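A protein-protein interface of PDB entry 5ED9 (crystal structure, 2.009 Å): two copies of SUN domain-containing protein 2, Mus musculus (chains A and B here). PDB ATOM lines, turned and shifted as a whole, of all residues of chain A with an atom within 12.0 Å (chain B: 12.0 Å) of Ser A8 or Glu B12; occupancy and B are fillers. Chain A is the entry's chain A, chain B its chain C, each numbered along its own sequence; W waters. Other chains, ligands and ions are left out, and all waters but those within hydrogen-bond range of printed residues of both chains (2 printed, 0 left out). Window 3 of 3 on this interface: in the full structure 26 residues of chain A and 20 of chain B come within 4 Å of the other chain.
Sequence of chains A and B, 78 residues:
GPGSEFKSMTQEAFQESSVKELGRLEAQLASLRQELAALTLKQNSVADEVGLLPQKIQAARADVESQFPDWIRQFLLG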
ATOM      1  N   PHE A   6      -3.873 -23.311 -26.084  1.00  0.00           N
ATOM      2  CA  PHE A   6      -5.257 -22.904 -26.315  1.00  0.00           C
ATOM      3  C   PHE A   6      -5.405 -21.385 -26.418  1.00  0.00           C
ATOM      4  O   PHE A   6      -4.804 -20.634 -25.647  1.00  0.00           O
ATOM      5  CB  PHE A   6      -6.184 -23.451 -25.220  1.00  0.00           C
ATOM      6  CG  PHE A   6      -7.606 -22.974 -25.339  1.00  0.00           C
ATOM      7  CD1 PHE A   6      -8.481 -23.577 -26.232  1.00  0.00           C
ATOM      8  CD2 PHE A   6      -8.064 -21.915 -24.563  1.00  0.00           C
ATOM      9  CE1 PHE A   6      -9.790 -23.136 -26.352  1.00  0.00           C
ATOM     10  CE2 PHE A   6      -9.370 -21.467 -24.677  1.00  0.00           C
ATOM     11  CZ  PHE A   6     -10.237 -22.080 -25.573  1.00  0.00           C
ATOM     12  N   LYS A   7      -6.220 -20.948 -27.373  1.00  0.00           N
ATOM     13  CA  LYS A   7      -6.451 -19.525 -27.606  1.00  0.00           C
ATOM     14  C   LYS A   7      -7.807 -19.089 -27.069  1.00  0.00           C
ATOM     15  O   LYS A   7      -8.842 -19.547 -27.545  1.00  0.00           O
ATOM     16  CB  LYS A   7      -6.398 -19.213 -29.103  1.00  0.00           C
ATOM     17  CG  LYS A   7      -6.664 -17.747 -29.421  1.00  0.00           C
ATOM     18  CD  LYS A   7      -7.299 -17.569 -30.790  1.00  0.00           C
ATOM     19  CE  LYS A   7      -7.427 -16.095 -31.146  1.00  0.00           C
ATOM     20  NZ  LYS A   7      -8.080 -15.888 -32.472  1.00  0.00           N
ATOM     21  N   SER A   8      -7.807 -18.196 -26.088  1.00  0.00           N
ATOM     22  CA  SER A   8      -9.065 -17.683 -25.570  1.00  0.00           C
ATOM     23  C   SER A   8      -9.520 -16.462 -26.358  1.00  0.00           C
ATOM     24  O   SER A   8      -8.704 -15.735 -26.919  1.00  0.00           O
ATOM     25  CB  SER A   8      -8.940 -17.334 -24.090  1.00  0.00           C
ATOM     26  OG  SER A   8      -8.060 -16.243 -23.896  1.00  0.00           O
ATOM     27  N   MET A   9     -10.832 -16.256 -26.400  1.00  0.00           N
ATOM     28  CA  MET A   9     -11.418 -15.068 -27.007  1.00  0.00           C
ATOM     29  C   MET A   9     -11.798 -14.114 -25.880  1.00  0.00           C
ATOM     30  O   MET A   9     -11.738 -14.482 -24.708  1.00  0.00           O
ATOM     31  CB  MET A   9     -12.677 -15.445 -27.803  1.00  0.00           C
ATOM     32  CG  MET A   9     -12.531 -16.671 -28.697  1.00  0.00           C
ATOM     33  SD  MET A   9     -14.119 -17.477 -29.052  1.00  0.00           S
ATOM     34  CE  MET A   9     -14.848 -16.339 -30.223  1.00  0.00           C
ATOM     35  N   THR A  10     -12.194 -12.893 -26.220  1.00  0.00           N
ATOM     36  CA  THR A  10     -12.740 -11.989 -25.213  1.00  0.00           C
ATOM     37  C   THR A  10     -14.057 -12.576 -24.727  1.00  0.00           C
ATOM     38  O   THR A  10     -14.628 -13.431 -25.396  1.00  0.00           O
ATOM     39  CB  THR A  10     -13.014 -10.590 -25.792  1.00  0.00           C
ATOM     40  OG1 THR A  10     -13.999 -10.695 -26.825  1.00  0.00           O
ATOM     41  CG2 THR A  10     -11.739  -9.980 -26.367  1.00  0.00           C
ATOM     42  N   GLN A  11     -14.530 -12.134 -23.564  1.00  0.00           N
ATOM     43  CA  GLN A  11     -15.826 -12.593 -23.053  1.00  0.00           C
ATOM     44  C   GLN A  11     -16.953 -12.362 -24.055  1.00  0.00           C
ATOM     45  O   GLN A  11     -17.810 -13.220 -24.249  1.00  0.00           O
ATOM     46  CB  GLN A  11     -16.176 -11.903 -21.732  1.00  0.00           C
ATOM     47  CG  GLN A  11     -15.393 -12.384 -20.519  1.00  0.00           C
ATOM     48  CD  GLN A  11     -15.970 -11.845 -19.228  1.00  0.00           C
ATOM     49  OE1 GLN A  11     -17.136 -12.089 -18.909  1.00  0.00           O
ATOM     50  NE2 GLN A  11     -15.170 -11.078 -18.489  1.00  0.00           N
ATOM     51  N   GLU A  12     -16.945 -11.194 -24.694  1.00  0.00           N
ATOM     52  CA  GLU A  12     -18.000 -10.837 -25.630  1.00  0.00           C
ATOM     53  C   GLU A  12     -17.975 -11.712 -26.884  1.00  0.00           C
ATOM     54  O   GLU A  12     -19.022 -12.159 -27.343  1.00  0.00           O
ATOM     55  CB  GLU A  12     -17.925  -9.351 -26.002  1.00  0.00           C
ATOM     56  CG  GLU A  12     -18.947  -8.920 -27.049  1.00  0.00           C
ATOM     57  CD  GLU A  12     -19.055  -7.407 -27.189  1.00  0.00           C
ATOM     58  OE1 GLU A  12     -19.656  -6.945 -28.185  1.00  0.00           O
ATOM     59  OE2 GLU A  12     -18.548  -6.681 -26.305  1.00  0.00           O
ATOM     60  N   ALA A  13     -16.787 -11.960 -27.427  1.00  0.00           N
ATOM     61  CA  ALA A  13     -16.651 -12.834 -28.591  1.00  0.00           C
ATOM     62  C   ALA A  13     -17.087 -14.267 -28.275  1.00  0.00           C
ATOM     63  O   ALA A  13     -17.745 -14.920 -29.090  1.00  0.00           O
ATOM     64  CB  ALA A  13     -15.226 -12.830 -29.092  1.00  0.00           C
ATOM     65  N   PHE A  14     -16.707 -14.768 -27.105  1.00  0.00           N
ATOM     66  CA  PHE A  14     -17.102 -16.123 -26.742  1.00  0.00           C
ATOM     67  C   PHE A  14     -18.605 -16.236 -26.499  1.00  0.00           C
ATOM     68  O   PHE A  14     -19.216 -17.252 -26.843  1.00  0.00           O
ATOM     69  CB  PHE A  14     -16.320 -16.659 -25.544  1.00  0.00           C
ATOM     70  CG  PHE A  14     -16.475 -18.134 -25.361  1.00  0.00           C
ATOM     71  CD1 PHE A  14     -15.801 -19.013 -26.189  1.00  0.00           C
ATOM     72  CD2 PHE A  14     -17.312 -18.647 -24.387  1.00  0.00           C
ATOM     73  CE1 PHE A  14     -15.954 -20.383 -26.050  1.00  0.00           C
ATOM     74  CE2 PHE A  14     -17.464 -20.022 -24.237  1.00  0.00           C
ATOM     75  CZ  PHE A  14     -16.786 -20.888 -25.072  1.00  0.00           C
ATOM     76  N   GLN A  15     -19.194 -15.199 -25.913  1.00  0.00           N
ATOM     77  CA  GLN A  15     -20.646 -15.130 -25.736  1.00  0.00           C
ATOM     78  C   GLN A  15     -21.349 -15.262 -27.081  1.00  0.00           C
ATOM     79  O   GLN A  15     -22.301 -16.029 -27.228  1.00  0.00           O
ATOM     80  CB  GLN A  15     -21.062 -13.809 -25.065  1.00  0.00           C
ATOM     81  CG  GLN A  15     -20.817 -13.737 -23.547  1.00  0.00           C
ATOM     82  CD  GLN A  15     -20.865 -12.306 -23.004  1.00  0.00           C
ATOM     83  OE1 GLN A  15     -21.298 -11.383 -23.687  1.00  0.00           O
ATOM     84  NE2 GLN A  15     -20.410 -12.128 -21.772  1.00  0.00           N
ATOM     85  N   GLU A  16     -20.867 -14.518 -28.069  1.00  0.00           N
ATOM     86  CA  GLU A  16     -21.490 -14.528 -29.385  1.00  0.00           C
ATOM     87  C   GLU A  16     -21.276 -15.858 -30.101  1.00  0.00           C
ATOM     88  O   GLU A  16     -22.210 -16.420 -30.665  1.00  0.00           O
ATOM     89  CB  GLU A  16     -20.967 -13.363 -30.232  1.00  0.00           C
ATOM     90  CG  GLU A  16     -21.238 -11.995 -29.619  1.00  0.00           C
ATOM     91  CD  GLU A  16     -20.699 -10.845 -30.465  1.00  0.00           C
ATOM     92  OE1 GLU A  16     -20.058 -11.106 -31.507  1.00  0.00           O
ATOM     93  OE2 GLU A  16     -20.921  -9.675 -30.084  1.00  0.00           O
ATOM     94  N   SER A  17     -20.053 -16.369 -30.079  1.00  0.00           N
ATOM     95  CA  SER A  17     -19.760 -17.592 -30.812  1.00  0.00           C
ATOM     96  C   SER A  17     -20.420 -18.834 -30.191  1.00  0.00           C
ATOM     97  O   SER A  17     -21.000 -19.657 -30.902  1.00  0.00           O
ATOM     98  CB  SER A  17     -18.251 -17.797 -30.993  1.00  0.00           C
ATOM     99  OG  SER A  17     -17.587 -17.907 -29.751  1.00  0.00           O
ATOM    100  N   SER A  18     -20.338 -18.965 -28.871  1.00  0.00           N
ATOM    101  CA  SER A  18     -20.854 -20.159 -28.212  1.00  0.00           C
ATOM    102  C   SER A  18     -22.370 -20.244 -28.327  1.00  0.00           C
ATOM    103  O   SER A  18     -22.927 -21.321 -28.522  1.00  0.00           O
ATOM    104  CB  SER A  18     -20.420 -20.205 -26.743  1.00  0.00           C
ATOM    105  OG  SER A  18     -20.982 -19.133 -26.006  1.00  0.00           O
ATOM    106  N   PHE B   6       0.576 -12.682 -11.505  1.00  0.00           N
ATOM    107  CA  PHE B   6      -0.253 -13.882 -11.553  1.00  0.00           C
ATOM    108  C   PHE B   6      -1.324 -13.790 -12.630  1.00  0.00           C
ATOM    109  O   PHE B   6      -2.078 -12.819 -12.679  1.00  0.00           O
ATOM    110  CB  PHE B   6      -0.897 -14.148 -10.188  1.00  0.00           C
ATOM    111  CG  PHE B   6      -2.035 -15.133 -10.235  1.00  0.00           C
ATOM    112  CD1 PHE B   6      -1.791 -16.500 -10.227  1.00  0.00           C
ATOM    113  CD2 PHE B   6      -3.353 -14.692 -10.285  1.00  0.00           C
ATOM    114  CE1 PHE B   6      -2.839 -17.407 -10.272  1.00  0.00           C
ATOM    115  CE2 PHE B   6      -4.401 -15.594 -10.335  1.00  0.00           C
ATOM    116  CZ  PHE B   6      -4.144 -16.954 -10.328  1.00  0.00           C
ATOM    117  N   LYS B   7      -1.396 -14.811 -13.480  1.00  0.00           N
ATOM    118  CA  LYS B   7      -2.406 -14.863 -14.535  1.00  0.00           C
ATOM    119  C   LYS B   7      -3.609 -15.701 -14.112  1.00  0.00           C
ATOM    120  O   LYS B   7      -3.475 -16.882 -13.802  1.00  0.00           O
ATOM    121  CB  LYS B   7      -1.802 -15.429 -15.822  1.00  0.00           C
ATOM    122  CG  LYS B   7      -0.541 -14.711 -16.261  1.00  0.00           C
ATOM    123  CD  LYS B   7       0.146 -15.422 -17.409  1.00  0.00           C
ATOM    124  CE  LYS B   7       1.468 -14.750 -17.740  1.00  0.00           C
ATOM    125  NZ  LYS B   7       1.285 -13.299 -18.020  1.00  0.00           N
ATOM    126  N   SER B   8      -4.786 -15.085 -14.088  1.00  0.00           N
ATOM    127  CA  SER B   8      -6.003 -15.803 -13.742  1.00  0.00           C
ATOM    128  C   SER B   8      -6.372 -16.731 -14.895  1.00  0.00           C
ATOM    129  O   SER B   8      -6.103 -16.424 -16.057  1.00  0.00           O
ATOM    130  CB  SER B   8      -7.136 -14.827 -13.453  1.00  0.00           C
ATOM    131  OG  SER B   8      -7.293 -13.918 -14.526  1.00  0.00           O
ATOM    132  N   MET B   9      -6.986 -17.868 -14.574  1.00  0.00           N
ATOM    133  CA  MET B   9      -7.180 -18.913 -15.569  1.00  0.00           C
ATOM    134  C   MET B   9      -8.612 -19.415 -15.693  1.00  0.00           C
ATOM    135  O   MET B   9      -8.902 -20.231 -16.566  1.00  0.00           O
ATOM    136  CB  MET B   9      -6.251 -20.092 -15.266  1.00  0.00           C
ATOM    137  CG  MET B   9      -4.804 -19.688 -14.965  1.00  0.00           C
ATOM    138  SD  MET B   9      -3.667 -19.788 -16.373  1.00  0.00           S
ATOM    139  CE  MET B   9      -4.223 -18.451 -17.433  1.00  0.00           C
ATOM    140  N   THR B  10      -9.504 -18.946 -14.823  1.00  0.00           N
ATOM    141  CA  THR B  10     -10.879 -19.455 -14.810  1.00  0.00           C
ATOM    142  C   THR B  10     -11.574 -19.282 -16.159  1.00  0.00           C
ATOM    143  O   THR B  10     -12.179 -20.223 -16.681  1.00  0.00           O
ATOM    144  CB  THR B  10     -11.727 -18.793 -13.711  1.00  0.00           C
ATOM    145  OG1 THR B  10     -11.275 -19.232 -12.424  1.00  0.00           O
ATOM    146  CG2 THR B  10     -13.185 -19.162 -13.879  1.00  0.00           C
ATOM    147  N   GLN B  11     -11.467 -18.082 -16.722  1.00  0.00           N
ATOM    148  CA  GLN B  11     -12.095 -17.753 -18.004  1.00  0.00           C
ATOM    149  C   GLN B  11     -11.596 -18.655 -19.130  1.00  0.00           C
ATOM    150  O   GLN B  11     -12.393 -19.217 -19.888  1.00  0.00           O
ATOM    151  CB  GLN B  11     -11.840 -16.280 -18.352  1.00  0.00           C
ATOM    152  CG  GLN B  11     -12.470 -15.801 -19.664  1.00  0.00           C
ATOM    153  CD  GLN B  11     -12.214 -14.322 -19.929  1.00  0.00           C
ATOM    154  OE1 GLN B  11     -11.991 -13.547 -19.001  1.00  0.00           O
ATOM    155  NE2 GLN B  11     -12.243 -13.928 -21.200  1.00  0.00           N
ATOM    156  N   GLU B  12     -10.280 -18.809 -19.233  1.00  0.00           N
ATOM    157  CA  GLU B  12      -9.705 -19.606 -20.311  1.00  0.00           C
ATOM    158  C   GLU B  12      -9.973 -21.094 -20.131  1.00  0.00           C
ATOM    159  O   GLU B  12     -10.106 -21.828 -21.109  1.00  0.00           O
ATOM    160  CB  GLU B  12      -8.207 -19.336 -20.470  1.00  0.00           C
ATOM    161  CG  GLU B  12      -7.884 -17.883 -20.824  1.00  0.00           C
ATOM    162  CD  GLU B  12      -6.476 -17.694 -21.365  1.00  0.00           C
ATOM    163  OE1 GLU B  12      -5.930 -18.635 -21.992  1.00  0.00           O
ATOM    164  OE2 GLU B  12      -5.918 -16.590 -21.174  1.00  0.00           O
ATOM    165  N   ALA B  13     -10.038 -21.544 -18.883  1.00  0.00           N
ATOM    166  CA  ALA B  13     -10.385 -22.938 -18.615  1.00  0.00           C
ATOM    167  C   ALA B  13     -11.859 -23.177 -18.924  1.00  0.00           C
ATOM    168  O   ALA B  13     -12.227 -24.226 -19.443  1.00  0.00           O
ATOM    169  CB  ALA B  13     -10.070 -23.314 -17.171  1.00  0.00           C
ATOM    170  N   PHE B  14     -12.699 -22.196 -18.611  1.00  0.00           N
ATOM    171  CA  PHE B  14     -14.128 -22.322 -18.876  1.00  0.00           C
ATOM    172  C   PHE B  14     -14.403 -22.350 -20.372  1.00  0.00           C
ATOM    173  O   PHE B  14     -15.240 -23.117 -20.840  1.00  0.00           O
ATOM    174  CB  PHE B  14     -14.932 -21.202 -18.211  1.00  0.00           C
ATOM    175  CG  PHE B  14     -16.376 -21.201 -18.608  1.00  0.00           C
ATOM    176  CD1 PHE B  14     -17.251 -22.129 -18.064  1.00  0.00           C
ATOM    177  CD2 PHE B  14     -16.851 -20.308 -19.555  1.00  0.00           C
ATOM    178  CE1 PHE B  14     -18.584 -22.155 -18.442  1.00  0.00           C
ATOM    179  CE2 PHE B  14     -18.180 -20.328 -19.939  1.00  0.00           C
ATOM    180  CZ  PHE B  14     -19.048 -21.253 -19.384  1.00  0.00           C
ATOM    181  N   GLN B  15     -13.690 -21.515 -21.124  1.00  0.00           N
ATOM    182  CA  GLN B  15     -13.828 -21.497 -22.575  1.00  0.00           C
ATOM    183  C   GLN B  15     -13.398 -22.814 -23.193  1.00  0.00           C
ATOM    184  O   GLN B  15     -14.111 -23.375 -24.018  1.00  0.00           O
ATOM    185  CB  GLN B  15     -13.044 -20.334 -23.193  1.00  0.00           C
ATOM    186  CG  GLN B  15     -13.683 -18.978 -22.949  1.00  0.00           C
ATOM    187  CD  GLN B  15     -12.996 -17.852 -23.709  1.00  0.00           C
ATOM    188  OE1 GLN B  15     -12.206 -18.091 -24.623  1.00  0.00           O
ATOM    189  NE2 GLN B  15     -13.298 -16.614 -23.329  1.00  0.00           N
ATOM    190  N   GLU B  16     -12.238 -23.313 -22.793  1.00  0.00           N
ATOM    191  CA  GLU B  16     -11.713 -24.549 -23.353  1.00  0.00           C
ATOM    192  C   GLU B  16     -12.621 -25.745 -23.043  1.00  0.00           C
ATOM    193  O   GLU B  16     -12.883 -26.575 -23.914  1.00  0.00           O
ATOM    194  CB  GLU B  16     -10.300 -24.804 -22.837  1.00  0.00           C
ATOM    195  CG  GLU B  16      -9.703 -26.127 -23.276  1.00  0.00           C
ATOM    196  CD  GLU B  16      -8.200 -26.190 -23.058  1.00  0.00           C
ATOM    197  OE1 GLU B  16      -7.650 -25.295 -22.382  1.00  0.00           O
ATOM    198  OE2 GLU B  16      -7.565 -27.137 -23.571  1.00  0.00           O
ATOM    199  N   SER B  17     -13.109 -25.826 -21.810  1.00  0.00           N
ATOM    200  CA  SER B  17     -13.959 -26.953 -21.423  1.00  0.00           C
ATOM    201  C   SER B  17     -15.318 -26.926 -22.122  1.00  0.00           C
ATOM    202  O   SER B  17     -15.828 -27.970 -22.546  1.00  0.00           O
ATOM    203  CB  SER B  17     -14.132 -27.018 -19.899  1.00  0.00           C
ATOM    204  OG  SER B  17     -14.764 -25.855 -19.391  1.00  0.00           O
ATOM    205  N   SER B  18     -15.895 -25.732 -22.241  1.00  0.00           N
ATOM    206  CA  SER B  18     -17.194 -25.552 -22.883  1.00  0.00           C
ATOM    207  C   SER B  18     -17.136 -25.919 -24.360  1.00  0.00           C
ATOM    208  O   SER B  18     -18.030 -26.598 -24.872  1.00  0.00           O
ATOM    209  CB  SER B  18     -17.667 -24.107 -22.732  1.00  0.00           C
ATOM    210  OG  SER B  18     -17.924 -23.797 -21.373  1.00  0.00           O
ATOM    211  N   VAL B  19     -16.091 -25.446 -25.039  1.00  0.00           N
ATOM    212  CA  VAL B  19     -15.860 -25.773 -26.439  1.00  0.00           C
ATOM    213  C   VAL B  19     -15.729 -27.273 -26.622  1.00  0.00           C
ATOM    214  O   VAL B  19     -16.335 -27.856 -27.522  1.00  0.00           O
ATOM    215  CB  VAL B  19     -14.564 -25.124 -26.970  1.00  0.00           C
ATOM    216  CG1 VAL B  19     -14.187 -25.732 -28.323  1.00  0.00           C
ATOM    217  CG2 VAL B  19     -14.722 -23.620 -27.086  1.00  0.00           C
ATOM    218  N   LYS B  20     -14.926 -27.887 -25.760  1.00  0.00           N
ATOM    219  CA  LYS B  20     -14.693 -29.322 -25.796  1.00  0.00           C
ATOM    220  C   LYS B  20     -15.972 -30.115 -25.517  1.00  0.00           C
ATOM    221  O   LYS B  20     -16.226 -31.144 -26.149  1.00  0.00           O
ATOM    222  CB  LYS B  20     -13.619 -29.695 -24.774  1.00  0.00           C
ATOM    223  CG  LYS B  20     -13.280 -31.169 -24.751  1.00  0.00           C
ATOM    224  CD  LYS B  20     -12.185 -31.494 -23.737  1.00  0.00           C
ATOM    225  CE  LYS B  20     -11.769 -32.967 -23.851  1.00  0.00           C
ATOM    226  NZ  LYS B  20     -10.603 -33.313 -22.979  1.00  0.00           N
ATOM    227  N   GLU B  21     -16.769 -29.644 -24.564  1.00  0.00           N
ATOM    228  CA  GLU B  21     -18.023 -30.314 -24.220  1.00  0.00           C
ATOM    229  C   GLU B  21     -19.024 -30.220 -25.370  1.00  0.00           C
ATOM    230  O   GLU B  21     -19.722 -31.188 -25.670  1.00  0.00           O
ATOM    231  CB  GLU B  21     -18.621 -29.757 -22.920  1.00  0.00           C
ATOM    232  CG  GLU B  21     -20.034 -30.281 -22.576  1.00  0.00           C
ATOM    233  CD  GLU B  21     -20.081 -31.759 -22.180  1.00  0.00           C
ATOM    234  OE1 GLU B  21     -19.056 -32.454 -22.281  1.00  0.00           O
ATOM    235  OE2 GLU B  21     -21.159 -32.238 -21.762  1.00  0.00           O
HETATM  236  O   HOH W   1     -12.716 -19.643 -27.345  1.00  0.00           O
HETATM  237  O   HOH W   2     -12.417 -10.609 -21.872  1.00  0.00           O
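Water W1 bridges the side-chain sulfur of Met A9 (3.1 Å) and the side-chain amide oxygen of Gln B15 (3.2 Å).
Water W2 lies within hydrogen-bond range of the backbone NH (N) of Gln A11 and the side-chain amide nitrogen (NE2) of Gln B11.
Among the printed residues, pairs that only touch across the chains: Phe A6 with Glu B12, Phe A6 with Glu B16, Ser A8 with Gln B15, Met A9 with Gln B11, Gln A11 with Gln B11, Phe A14 with Gln B15 and Phe A14 with Val B19.
Phe A6 touches Glu B12, but with the chains exchanged Glu A12 does not touch Phe B6 (19.2 Å).
Phe A6 touches Glu B16, but with the chains exchanged Glu A16 does not touch Phe B6 (24.2 Å).
Ser A8 touches Gln B15, but with the chains exchanged Gln A15 does not touch Ser B8 (15.1 Å).
Gln B11 touches its own counterpart, Gln A11.
Hydrophobic or aromatic side chains of chain A that line the printed part of chain B: Phe A6 and Phe A14.
Among the printed residues, 9 pairs touch across the chains.
The backbone NH (N) of Met A9 sits at hydrogen-bond distance from the side-chain amide oxygen (OE1) of Gln B15 (2.9 Å).
The side-chain carboxylate of Glu B12 sits close to the side-chain hydroxyl of Ser A8.
OG of Ser A17 lies within hydrogen-bond range of O of Phe A14.
OG of Ser A17 sits close to SD of Met A9, at 3.6 Å.
The backbone carbonyl oxygen (O) of Phe A14 is in hydrogen-bond range of the side-chain hydroxyl (OG) of Ser A18, 2.7 Å away.
Ser A8 touches just these residues of chain B: Glu B12 and Gln B15.
Of chain A, only Phe A6 (3.7 Å) and Ser A8 (3.3 Å) come within 4 Å of Glu B12.
Of chain B, only Glu B12 and Glu B16 come within 4 Å of Phe A6.
Lys A7 touches none of the printed residues of chain B.
Met A9 touches just these residues of chain B: Gln B11 and Gln B15.
No residue of chain A comes within 4 Å of Ser B8.
No residue of chain A comes within 4 Å of Met B9.
No residue of chain A comes within 4 Å of Thr B10.
Gln B11 touches just these residues of chain A: Met A9 and Gln A11.
No residue of chain A comes within 4 Å of Ala B13.
Glu B16 touches one residue of chain A.
Of the printed residues of chain B, Phe A14 touches Gln B15 and Val B19.
Of the printed residues of chain A, Val B19 touches Phe A14.
Of the printed residues of chain B, Gln A11 touches Gln B11.
The nearest residue of chain B that does not touch Ser A8 is Gln B11 (5.5 Å).
The nearest residue of chain A that does not touch Glu B12 is Lys A7 (5.4 Å).
The nearest printed residue of chain B that does not touch Phe A14 is Ser B18 (4.1 Å).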
